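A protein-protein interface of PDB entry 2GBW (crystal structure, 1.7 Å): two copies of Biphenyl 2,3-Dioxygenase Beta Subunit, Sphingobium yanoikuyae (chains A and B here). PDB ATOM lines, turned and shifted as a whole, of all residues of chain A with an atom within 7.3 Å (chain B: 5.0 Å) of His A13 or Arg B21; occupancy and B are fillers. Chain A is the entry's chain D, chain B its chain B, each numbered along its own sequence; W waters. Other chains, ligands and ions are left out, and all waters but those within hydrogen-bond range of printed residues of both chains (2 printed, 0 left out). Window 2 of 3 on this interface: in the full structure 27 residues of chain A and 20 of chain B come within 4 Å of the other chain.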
ATOM      1  N   VAL A   8      17.831  16.914  -6.761  1.00  0.00           N
ATOM      2  CA  VAL A   8      17.145  16.532  -8.005  1.00  0.00           C
ATOM      3  C   VAL A   8      16.706  17.754  -8.779  1.00  0.00           C
ATOM      4  O   VAL A   8      16.595  18.857  -8.249  1.00  0.00           O
ATOM      5  CB  VAL A   8      15.954  15.603  -7.735  1.00  0.00           C
ATOM      6  CG1 VAL A   8      16.449  14.351  -7.020  1.00  0.00           C
ATOM      7  CG2 VAL A   8      14.882  16.321  -6.957  1.00  0.00           C
ATOM      8  N   THR A   9      16.447  17.549 -10.066  1.00  0.00           N
ATOM      9  CA  THR A   9      15.890  18.602 -10.895  1.00  0.00           C
ATOM     10  C   THR A   9      14.472  18.880 -10.484  1.00  0.00           C
ATOM     11  O   THR A   9      13.809  18.047  -9.840  1.00  0.00           O
ATOM     12  CB  THR A   9      15.894  18.224 -12.395  1.00  0.00           C
ATOM     13  OG1 THR A   9      15.023  17.091 -12.613  1.00  0.00           O
ATOM     14  CG2 THR A   9      17.344  17.905 -12.930  1.00  0.00           C
ATOM     15  N   PRO A  10      13.975  20.077 -10.820  1.00  0.00           N
ATOM     16  CA  PRO A  10      12.592  20.424 -10.515  1.00  0.00           C
ATOM     17  C   PRO A  10      11.535  19.451 -11.090  1.00  0.00           C
ATOM     18  O   PRO A  10      10.537  19.173 -10.405  1.00  0.00           O
ATOM     19  CB  PRO A  10      12.454  21.821 -11.134  1.00  0.00           C
ATOM     20  CG  PRO A  10      13.859  22.375 -11.046  1.00  0.00           C
ATOM     21  CD  PRO A  10      14.680  21.201 -11.483  1.00  0.00           C
ATOM     22  N   ASP A  11      11.737  18.916 -12.303  1.00  0.00           N
ATOM     23  CA  ASP A  11      10.789  17.921 -12.840  1.00  0.00           C
ATOM     24  C   ASP A  11      10.780  16.589 -12.052  1.00  0.00           C
ATOM     25  O   ASP A  11       9.718  16.004 -11.808  1.00  0.00           O
ATOM     26  CB  ASP A  11      11.071  17.658 -14.292  1.00  0.00           C
ATOM     27  CG  ASP A  11      10.686  18.830 -15.183  1.00  0.00           C
ATOM     28  OD1 ASP A  11       9.931  19.728 -14.727  1.00  0.00           O
ATOM     29  OD2 ASP A  11      11.110  18.816 -16.348  1.00  0.00           O
ATOM     30  N   VAL A  12      11.957  16.134 -11.646  1.00  0.00           N
ATOM     31  CA  VAL A  12      12.049  14.976 -10.742  1.00  0.00           C
ATOM     32  C   VAL A  12      11.415  15.290  -9.411  1.00  0.00           C
ATOM     33  O   VAL A  12      10.671  14.467  -8.890  1.00  0.00           O
ATOM     34  CB  VAL A  12      13.528  14.477 -10.620  1.00  0.00           C
ATOM     35  CG1 VAL A  12      13.665  13.409  -9.514  1.00  0.00           C
ATOM     36  CG2 VAL A  12      13.996  13.928 -12.022  1.00  0.00           C
ATOM     37  N   HIS A  13      11.674  16.472  -8.869  1.00  0.00           N
ATOM     38  CA  HIS A  13      11.043  16.896  -7.630  1.00  0.00           C
ATOM     39  C   HIS A  13       9.535  16.757  -7.709  1.00  0.00           C
ATOM     40  O   HIS A  13       8.922  16.204  -6.789  1.00  0.00           O
ATOM     41  CB  HIS A  13      11.368  18.333  -7.276  1.00  0.00           C
ATOM     42  CG  HIS A  13      10.897  18.693  -5.893  1.00  0.00           C
ATOM     43  ND1 HIS A  13       9.656  19.219  -5.660  1.00  0.00           N
ATOM     44  CD2 HIS A  13      11.494  18.573  -4.686  1.00  0.00           C
ATOM     45  CE1 HIS A  13       9.509  19.438  -4.359  1.00  0.00           C
ATOM     46  NE2 HIS A  13      10.602  19.029  -3.746  1.00  0.00           N
ATOM     47  N   TYR A  14       8.970  17.296  -8.785  1.00  0.00           N
ATOM     48  CA  TYR A  14       7.560  17.212  -9.027  1.00  0.00           C
ATOM     49  C   TYR A  14       7.079  15.782  -8.918  1.00  0.00           C
ATOM     50  O   TYR A  14       6.092  15.509  -8.228  1.00  0.00           O
ATOM     51  CB  TYR A  14       7.144  17.814 -10.355  1.00  0.00           C
ATOM     52  CG  TYR A  14       5.637  17.772 -10.498  1.00  0.00           C
ATOM     53  CD1 TYR A  14       4.984  16.662 -11.027  1.00  0.00           C
ATOM     54  CD2 TYR A  14       4.863  18.825 -10.002  1.00  0.00           C
ATOM     55  CE1 TYR A  14       3.568  16.631 -11.090  1.00  0.00           C
ATOM     56  CE2 TYR A  14       3.485  18.803 -10.062  1.00  0.00           C
ATOM     57  CZ  TYR A  14       2.831  17.715 -10.598  1.00  0.00           C
ATOM     58  OH  TYR A  14       1.429  17.735 -10.650  1.00  0.00           O
ATOM     59  N   ASP A  15       7.736  14.863  -9.619  1.00  0.00           N
ATOM     60  CA  ASP A  15       7.229  13.498  -9.680  1.00  0.00           C
ATOM     61  C   ASP A  15       7.298  12.871  -8.295  1.00  0.00           C
ATOM     62  O   ASP A  15       6.436  12.081  -7.958  1.00  0.00           O
ATOM     63  CB  ASP A  15       7.999  12.673 -10.679  1.00  0.00           C
ATOM     64  CG  ASP A  15       7.603  12.979 -12.106  1.00  0.00           C
ATOM     65  OD1 ASP A  15       6.705  13.818 -12.309  1.00  0.00           O
ATOM     66  OD2 ASP A  15       8.175  12.355 -13.008  1.00  0.00           O
ATOM     67  N   ILE A  16       8.356  13.169  -7.540  1.00  0.00           N
ATOM     68  CA  ILE A  16       8.490  12.658  -6.180  1.00  0.00           C
ATOM     69  C   ILE A  16       7.365  13.171  -5.281  1.00  0.00           C
ATOM     70  O   ILE A  16       6.723  12.385  -4.572  1.00  0.00           O
ATOM     71  CB  ILE A  16       9.877  12.943  -5.577  1.00  0.00           C
ATOM     72  CG1 ILE A  16      10.935  12.148  -6.350  1.00  0.00           C
ATOM     73  CG2 ILE A  16       9.932  12.532  -4.055  1.00  0.00           C
ATOM     74  CD1 ILE A  16      12.329  12.575  -5.980  1.00  0.00           C
ATOM     75  N   GLU A  17       7.098  14.464  -5.320  1.00  0.00           N
ATOM     76  CA  GLU A  17       5.951  15.019  -4.552  1.00  0.00           C
ATOM     77  C   GLU A  17       4.599  14.380  -4.947  1.00  0.00           C
ATOM     78  O   GLU A  17       3.771  14.067  -4.071  1.00  0.00           O
ATOM     79  CB  GLU A  17       5.863  16.537  -4.739  1.00  0.00           C
ATOM     80  CG  GLU A  17       6.985  17.350  -4.090  1.00  0.00           C
ATOM     81  CD  GLU A  17       6.577  18.196  -2.888  1.00  0.00           C
ATOM     82  OE1 GLU A  17       5.617  17.829  -2.152  1.00  0.00           O
ATOM     83  OE2 GLU A  17       7.261  19.232  -2.651  1.00  0.00           O
ATOM     84  N   ALA A  18       4.350  14.236  -6.245  1.00  0.00           N
ATOM     85  CA  ALA A  18       3.144  13.598  -6.750  1.00  0.00           C
ATOM     86  C   ALA A  18       3.028  12.167  -6.180  1.00  0.00           C
ATOM     87  O   ALA A  18       1.966  11.712  -5.785  1.00  0.00           O
ATOM     88  CB  ALA A  18       3.131  13.608  -8.350  1.00  0.00           C
ATOM     89  N   HIS A  19       4.138  11.442  -6.165  1.00  0.00           N
ATOM     90  CA  HIS A  19       4.142  10.091  -5.629  1.00  0.00           C
ATOM     91  C   HIS A  19       3.736  10.121  -4.133  1.00  0.00           C
ATOM     92  O   HIS A  19       2.875   9.354  -3.718  1.00  0.00           O
ATOM     93  CB  HIS A  19       5.518   9.464  -5.836  1.00  0.00           C
ATOM     94  CG  HIS A  19       5.701   8.176  -5.108  1.00  0.00           C
ATOM     95  ND1 HIS A  19       5.424   6.949  -5.681  1.00  0.00           N
ATOM     96  CD2 HIS A  19       6.183   7.918  -3.870  1.00  0.00           C
ATOM     97  CE1 HIS A  19       5.732   5.996  -4.815  1.00  0.00           C
ATOM     98  NE2 HIS A  19       6.192   6.558  -3.716  1.00  0.00           N
ATOM     99  N   ARG A  21       2.002  12.440  -2.560  1.00  0.00           N
ATOM    100  CA  ARG A  21       0.565  12.828  -2.456  1.00  0.00           C
ATOM    101  C   ARG A  21      -0.343  11.614  -2.693  1.00  0.00           C
ATOM    102  O   ARG A  21      -1.299  11.399  -1.965  1.00  0.00           O
ATOM    103  CB  ARG A  21       0.260  13.954  -3.442  1.00  0.00           C
ATOM    104  CG  ARG A  21       0.864  15.263  -3.008  1.00  0.00           C
ATOM    105  CD  ARG A  21       0.325  16.438  -3.761  1.00  0.00           C
ATOM    106  NE  ARG A  21       0.705  16.373  -5.164  1.00  0.00           N
ATOM    107  CZ  ARG A  21       1.719  17.061  -5.695  1.00  0.00           C
ATOM    108  NH1 ARG A  21       2.433  17.889  -4.937  1.00  0.00           N
ATOM    109  NH2 ARG A  21       1.975  16.973  -6.969  1.00  0.00           N
ATOM    110  N   SER A 104       5.579  17.902   4.236  1.00  0.00           N
ATOM    111  CA  SER A 104       6.203  19.162   3.873  1.00  0.00           C
ATOM    112  C   SER A 104       7.705  19.002   3.768  1.00  0.00           C
ATOM    113  O   SER A 104       8.268  17.993   4.156  1.00  0.00           O
ATOM    114  CB  SER A 104       5.863  20.247   4.899  1.00  0.00           C
ATOM    115  OG  SER A 104       4.474  20.564   4.896  1.00  0.00           O
ATOM    116  N   ASN A 105       8.346  19.981   3.134  1.00  0.00           N
ATOM    117  CA  ASN A 105       9.773  20.003   3.085  1.00  0.00           C
ATOM    118  C   ASN A 105      10.388  18.787   2.412  1.00  0.00           C
ATOM    119  O   ASN A 105      11.437  18.299   2.848  1.00  0.00           O
ATOM    120  CB  ASN A 105      10.410  20.200   4.461  1.00  0.00           C
ATOM    121  CG  ASN A 105      11.418  21.391   4.474  1.00  0.00           C
ATOM    122  OD1 ASN A 105      11.006  22.558   4.480  1.00  0.00           O
ATOM    123  ND2 ASN A 105      12.699  21.094   4.468  1.00  0.00           N
ATOM    124  N   VAL A 106       9.836  18.419   1.249  1.00  0.00           N
ATOM    125  CA  VAL A 106      10.357  17.266   0.534  1.00  0.00           C
ATOM    126  C   VAL A 106      11.641  17.701  -0.182  1.00  0.00           C
ATOM    127  O   VAL A 106      11.623  18.677  -0.924  1.00  0.00           O
ATOM    128  CB  VAL A 106       9.325  16.688  -0.421  1.00  0.00           C
ATOM    129  CG1 VAL A 106       9.923  15.506  -1.275  1.00  0.00           C
ATOM    130  CG2 VAL A 106       8.046  16.288   0.336  1.00  0.00           C
ATOM    131  N   GLU A 107      12.765  17.038   0.108  1.00  0.00           N
ATOM    132  CA  GLU A 107      14.029  17.317  -0.563  1.00  0.00           C
ATOM    133  C   GLU A 107      14.646  15.991  -1.014  1.00  0.00           C
ATOM    134  O   GLU A 107      14.811  15.080  -0.217  1.00  0.00           O
ATOM    135  CB  GLU A 107      14.977  18.039   0.367  1.00  0.00           C
ATOM    136  CG  GLU A 107      14.486  19.409   0.855  1.00  0.00           C
ATOM    137  CD  GLU A 107      15.573  20.083   1.704  1.00  0.00           C
ATOM    138  OE1 GLU A 107      15.733  19.659   2.860  1.00  0.00           O
ATOM    139  OE2 GLU A 107      16.274  20.988   1.218  1.00  0.00           O
ATOM    140  N   ALA A 108      14.951  15.886  -2.286  1.00  0.00           N
ATOM    141  CA  ALA A 108      15.489  14.661  -2.831  1.00  0.00           C
ATOM    142  C   ALA A 108      16.843  14.919  -3.419  1.00  0.00           C
ATOM    143  O   ALA A 108      17.136  16.017  -3.988  1.00  0.00           O
ATOM    144  CB  ALA A 108      14.572  14.070  -3.857  1.00  0.00           C
ATOM    145  N   LEU A 119      14.177  13.241   1.942  1.00  0.00           N
ATOM    146  CA  LEU A 119      13.828  13.718   3.248  1.00  0.00           C
ATOM    147  C   LEU A 119      12.463  14.393   3.210  1.00  0.00           C
ATOM    148  O   LEU A 119      12.104  15.010   2.212  1.00  0.00           O
ATOM    149  CB  LEU A 119      14.875  14.743   3.656  1.00  0.00           C
ATOM    150  CG  LEU A 119      16.319  14.279   3.616  1.00  0.00           C
ATOM    151  CD1 LEU A 119      17.199  15.465   4.027  1.00  0.00           C
ATOM    152  CD2 LEU A 119      16.484  13.036   4.505  1.00  0.00           C
ATOM    153  N   ASN A 121       9.244  16.181   6.055  1.00  0.00           N
ATOM    154  CA  ASN A 121       8.563  16.428   7.345  1.00  0.00           C
ATOM    155  C   ASN A 121       7.135  15.925   7.282  1.00  0.00           C
ATOM    156  O   ASN A 121       6.432  16.167   6.290  1.00  0.00           O
ATOM    157  CB  ASN A 121       8.529  17.931   7.653  1.00  0.00           C
ATOM    158  CG  ASN A 121       9.893  18.498   8.057  1.00  0.00           C
ATOM    159  OD1 ASN A 121      10.847  17.764   8.315  1.00  0.00           O
ATOM    160  ND2 ASN A 121       9.990  19.813   8.105  1.00  0.00           N
ATOM    161  N   PHE A 151       7.930   5.180  -8.743  1.00  0.00           N
ATOM    162  CA  PHE A 151       8.874   4.925  -7.676  1.00  0.00           C
ATOM    163  C   PHE A 151       8.314   3.848  -6.756  1.00  0.00           C
ATOM    164  O   PHE A 151       7.076   3.717  -6.570  1.00  0.00           O
ATOM    165  CB  PHE A 151       9.118   6.179  -6.830  1.00  0.00           C
ATOM    166  CG  PHE A 151       9.553   7.391  -7.614  1.00  0.00           C
ATOM    167  CD1 PHE A 151      10.841   7.521  -8.070  1.00  0.00           C
ATOM    168  CD2 PHE A 151       8.646   8.404  -7.881  1.00  0.00           C
ATOM    169  CE1 PHE A 151      11.223   8.656  -8.824  1.00  0.00           C
ATOM    170  CE2 PHE A 151       9.004   9.538  -8.606  1.00  0.00           C
ATOM    171  CZ  PHE A 151      10.307   9.656  -9.107  1.00  0.00           C
ATOM    172  N   TYR B  14       9.561  27.859  -7.900  1.00  0.00           N
ATOM    173  CA  TYR B  14      10.203  26.613  -7.492  1.00  0.00           C
ATOM    174  C   TYR B  14      11.507  26.906  -6.768  1.00  0.00           C
ATOM    175  O   TYR B  14      11.803  26.360  -5.688  1.00  0.00           O
ATOM    176  CB  TYR B  14      10.516  25.715  -8.707  1.00  0.00           C
ATOM    177  CG  TYR B  14      11.222  24.474  -8.219  1.00  0.00           C
ATOM    178  CD1 TYR B  14      10.487  23.361  -7.811  1.00  0.00           C
ATOM    179  CD2 TYR B  14      12.620  24.430  -8.094  1.00  0.00           C
ATOM    180  CE1 TYR B  14      11.110  22.229  -7.343  1.00  0.00           C
ATOM    181  CE2 TYR B  14      13.269  23.285  -7.628  1.00  0.00           C
ATOM    182  CZ  TYR B  14      12.504  22.192  -7.239  1.00  0.00           C
ATOM    183  OH  TYR B  14      13.071  21.034  -6.725  1.00  0.00           O
ATOM    184  N   GLU B  17      10.885  28.184  -3.194  1.00  0.00           N
ATOM    185  CA  GLU B  17      10.502  27.065  -2.352  1.00  0.00           C
ATOM    186  C   GLU B  17      11.698  26.164  -1.962  1.00  0.00           C
ATOM    187  O   GLU B  17      11.794  25.711  -0.795  1.00  0.00           O
ATOM    188  CB  GLU B  17       9.429  26.253  -3.062  1.00  0.00           C
ATOM    189  CG  GLU B  17       8.075  26.989  -3.078  1.00  0.00           C
ATOM    190  CD  GLU B  17       6.952  26.310  -2.309  1.00  0.00           C
ATOM    191  OE1 GLU B  17       7.195  25.705  -1.224  1.00  0.00           O
ATOM    192  OE2 GLU B  17       5.796  26.432  -2.803  1.00  0.00           O
ATOM    193  N   ALA B  18      12.548  25.846  -2.938  1.00  0.00           N
ATOM    194  CA  ALA B  18      13.724  25.043  -2.704  1.00  0.00           C
ATOM    195  C   ALA B  18      14.705  25.725  -1.717  1.00  0.00           C
ATOM    196  O   ALA B  18      15.239  25.072  -0.830  1.00  0.00           O
ATOM    197  CB  ALA B  18      14.408  24.729  -4.043  1.00  0.00           C
ATOM    198  N   HIS B  19      14.897  27.041  -1.861  1.00  0.00           N
ATOM    199  CA  HIS B  19      15.624  27.850  -0.900  1.00  0.00           C
ATOM    200  C   HIS B  19      15.037  27.742   0.532  1.00  0.00           C
ATOM    201  O   HIS B  19      15.777  27.494   1.474  1.00  0.00           O
ATOM    202  CB  HIS B  19      15.619  29.332  -1.330  1.00  0.00           C
ATOM    203  CG  HIS B  19      16.172  30.264  -0.299  1.00  0.00           C
ATOM    204  ND1 HIS B  19      17.522  30.546  -0.203  1.00  0.00           N
ATOM    205  CD2 HIS B  19      15.570  30.935   0.719  1.00  0.00           C
ATOM    206  CE1 HIS B  19      17.715  31.360   0.820  1.00  0.00           C
ATOM    207  NE2 HIS B  19      16.551  31.624   1.380  1.00  0.00           N
ATOM    208  N   TYR B  20      13.731  27.936   0.652  1.00  0.00           N
ATOM    209  CA  TYR B  20      13.055  27.815   1.936  1.00  0.00           C
ATOM    210  C   TYR B  20      13.163  26.406   2.531  1.00  0.00           C
ATOM    211  O   TYR B  20      13.357  26.265   3.732  1.00  0.00           O
ATOM    212  CB  TYR B  20      11.593  28.240   1.815  1.00  0.00           C
ATOM    213  CG  TYR B  20      11.333  29.733   1.891  1.00  0.00           C
ATOM    214  CD1 TYR B  20      12.293  30.614   2.356  1.00  0.00           C
ATOM    215  CD2 TYR B  20      10.112  30.255   1.504  1.00  0.00           C
ATOM    216  CE1 TYR B  20      12.038  31.975   2.428  1.00  0.00           C
ATOM    217  CE2 TYR B  20       9.855  31.600   1.578  1.00  0.00           C
ATOM    218  CZ  TYR B  20      10.821  32.460   2.035  1.00  0.00           C
ATOM    219  OH  TYR B  20      10.555  33.803   2.101  1.00  0.00           O
ATOM    220  N   ARG B  21      13.048  25.367   1.706  1.00  0.00           N
ATOM    221  CA  ARG B  21      13.198  23.965   2.201  1.00  0.00           C
ATOM    222  C   ARG B  21      14.597  23.723   2.734  1.00  0.00           C
ATOM    223  O   ARG B  21      14.762  23.109   3.792  1.00  0.00           O
ATOM    224  CB  ARG B  21      12.837  22.968   1.082  1.00  0.00           C
ATOM    225  CG  ARG B  21      11.338  22.861   0.821  1.00  0.00           C
ATOM    226  CD  ARG B  21      10.998  21.699  -0.163  1.00  0.00           C
ATOM    227  NE  ARG B  21      11.524  21.846  -1.505  1.00  0.00           N
ATOM    228  CZ  ARG B  21      10.831  22.289  -2.553  1.00  0.00           C
ATOM    229  NH1 ARG B  21       9.573  22.667  -2.417  1.00  0.00           N
ATOM    230  NH2 ARG B  21      11.393  22.359  -3.748  1.00  0.00           N
ATOM    231  N   ALA B  22      15.606  24.293   2.057  1.00  0.00           N
ATOM    232  CA  ALA B  22      17.007  24.152   2.515  1.00  0.00           C
ATOM    233  C   ALA B  22      17.236  24.894   3.813  1.00  0.00           C
ATOM    234  O   ALA B  22      17.970  24.398   4.703  1.00  0.00           O
ATOM    235  CB  ALA B  22      18.035  24.552   1.373  1.00  0.00           C
ATOM    236  N   GLU B  23      16.607  26.056   3.920  1.00  0.00           N
ATOM    237  CA  GLU B  23      16.641  26.856   5.131  1.00  0.00           C
ATOM    238  C   GLU B  23      16.086  26.072   6.316  1.00  0.00           C
ATOM    239  O   GLU B  23      16.741  25.926   7.332  1.00  0.00           O
ATOM    240  CB  GLU B  23      15.843  28.138   4.924  1.00  0.00           C
ATOM    241  CG  GLU B  23      15.823  29.063   6.109  1.00  0.00           C
ATOM    242  CD  GLU B  23      15.312  30.439   5.760  1.00  0.00           C
ATOM    243  OE1 GLU B  23      14.178  30.539   5.269  1.00  0.00           O
ATOM    244  OE2 GLU B  23      16.045  31.414   5.969  1.00  0.00           O
ATOM    245  N   VAL B  24      14.875  25.565   6.160  1.00  0.00           N
ATOM    246  CA  VAL B  24      14.279  24.694   7.157  1.00  0.00           C
ATOM    247  C   VAL B  24      15.211  23.557   7.569  1.00  0.00           C
ATOM    248  O   VAL B  24      15.359  23.264   8.743  1.00  0.00           O
ATOM    249  CB  VAL B  24      12.926  24.155   6.703  1.00  0.00           C
ATOM    250  CG1 VAL B  24      12.503  23.000   7.552  1.00  0.00           C
ATOM    251  CG2 VAL B  24      11.895  25.238   6.760  1.00  0.00           C
ATOM    252  N   ARG B  25      15.859  22.929   6.596  1.00  0.00           N
ATOM    253  CA  ARG B  25      16.758  21.830   6.906  1.00  0.00           C
ATOM    254  C   ARG B  25      17.929  22.295   7.775  1.00  0.00           C
ATOM    255  O   ARG B  25      18.356  21.588   8.677  1.00  0.00           O
ATOM    256  CB  ARG B  25      17.251  21.150   5.630  1.00  0.00           C
ATOM    257  CG  ARG B  25      17.793  19.748   5.811  1.00  0.00           C
ATOM    258  CD  ARG B  25      18.253  19.168   4.463  1.00  0.00           C
ATOM    259  NE  ARG B  25      19.593  19.625   4.106  1.00  0.00           N
ATOM    260  CZ  ARG B  25      19.923  20.236   2.973  1.00  0.00           C
ATOM    261  NH1 ARG B  25      19.021  20.482   2.032  1.00  0.00           N
ATOM    262  NH2 ARG B  25      21.173  20.611   2.786  1.00  0.00           N
HETATM  263  O   HOH W   1      16.047  22.451  -1.080  1.00  0.00           O
HETATM  264  O   HOH W   2      15.657  20.522  -6.309  1.00  0.00           O
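Printed residues of chain B within 4 Å of Pro A10: Tyr B14. Of chain B, only Tyr B14 (3.2 Å) and Arg B21 (3.4 Å) come within 4 Å of His A13. Asp A15 touches none of the printed residues of chain B. Of the printed residues of chain B, Val A106 touches Arg B21 (3.2 Å). Asn A121 touches none of the printed residues of chain B. Arg B21 touches just these residues of chain A: His A13 (3.4 Å), Asn A105 (3.0 Å), Val A106 (3.2 Å) and Glu A107 (3.5 Å). Of the printed residues of chain A, Arg B25 touches Glu A107 and Leu A119. The nearest printed residue of chain B that does not touch His A13 is Ala B18 (6.8 Å).
Water W2 lies within hydrogen-bond range of OH of Tyr B14 and O of Val A8. Water W1 bridges OE2 of Glu A107 (2.7 Å) and O of Ala B18 (2.8 Å).
5 positions are printed for both chains. Of the 10 pairs that touch across the chains among the printed residues, none has its exchanged pair printed and touching as well.
Printed residues of chain A that touch a printed residue of chain B: Pro A10, His A13, Asn A105, Val A106, Glu A107 and Leu A119. Hydrophobic or aromatic side chains of chain A within 4 Å of the printed part of chain B: Pro A10, His A13 and Leu A119. Hydrophobic or aromatic side chains of chain B within 4 Å of the printed part of chain A: Tyr B14, Ala B22 and Val B24.
The guanidinium group (NH2) of Arg B21 is in hydrogen-bond range of a ring nitrogen (NE2) of His A13, 3.4 Å away. The backbone carbonyl oxygen (O) of Arg B21 sits at hydrogen-bond distance from the side-chain amide nitrogen (ND2) of Asn A105, at 3.0 Å. The guanidinium group (NE) of Arg B21 lies close to the backbone carbonyl oxygen (O) of Val A106 (3.2 Å). The backbone NH (N) of Ala B22 is in hydrogen-bond range of the side-chain carboxylate (OE2) of Glu A107 (3.5 Å). OE2 of Glu A107 lies within salt-bridge range of NH1 of Arg B25, at 2.9 Å.
A ring nitrogen (NE2) of His A13 lies within hydrogen-bond range of the backbone carbonyl oxygen of Val A106 (3.0 Å). O of Glu A107 is in hydrogen-bond range of N of Leu A119, at 2.9 Å.
Tyr B14 touches Pro A10 (CE2 to CG, 3.6 Å). Tyr B14 touches His A13. Asn A105 touches Val B24 (OD1 to CB, 3.3 Å). Glu A107 touches Arg B21. Arg B25 touches Leu A119 (CD to CD1, 3.9 Å).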
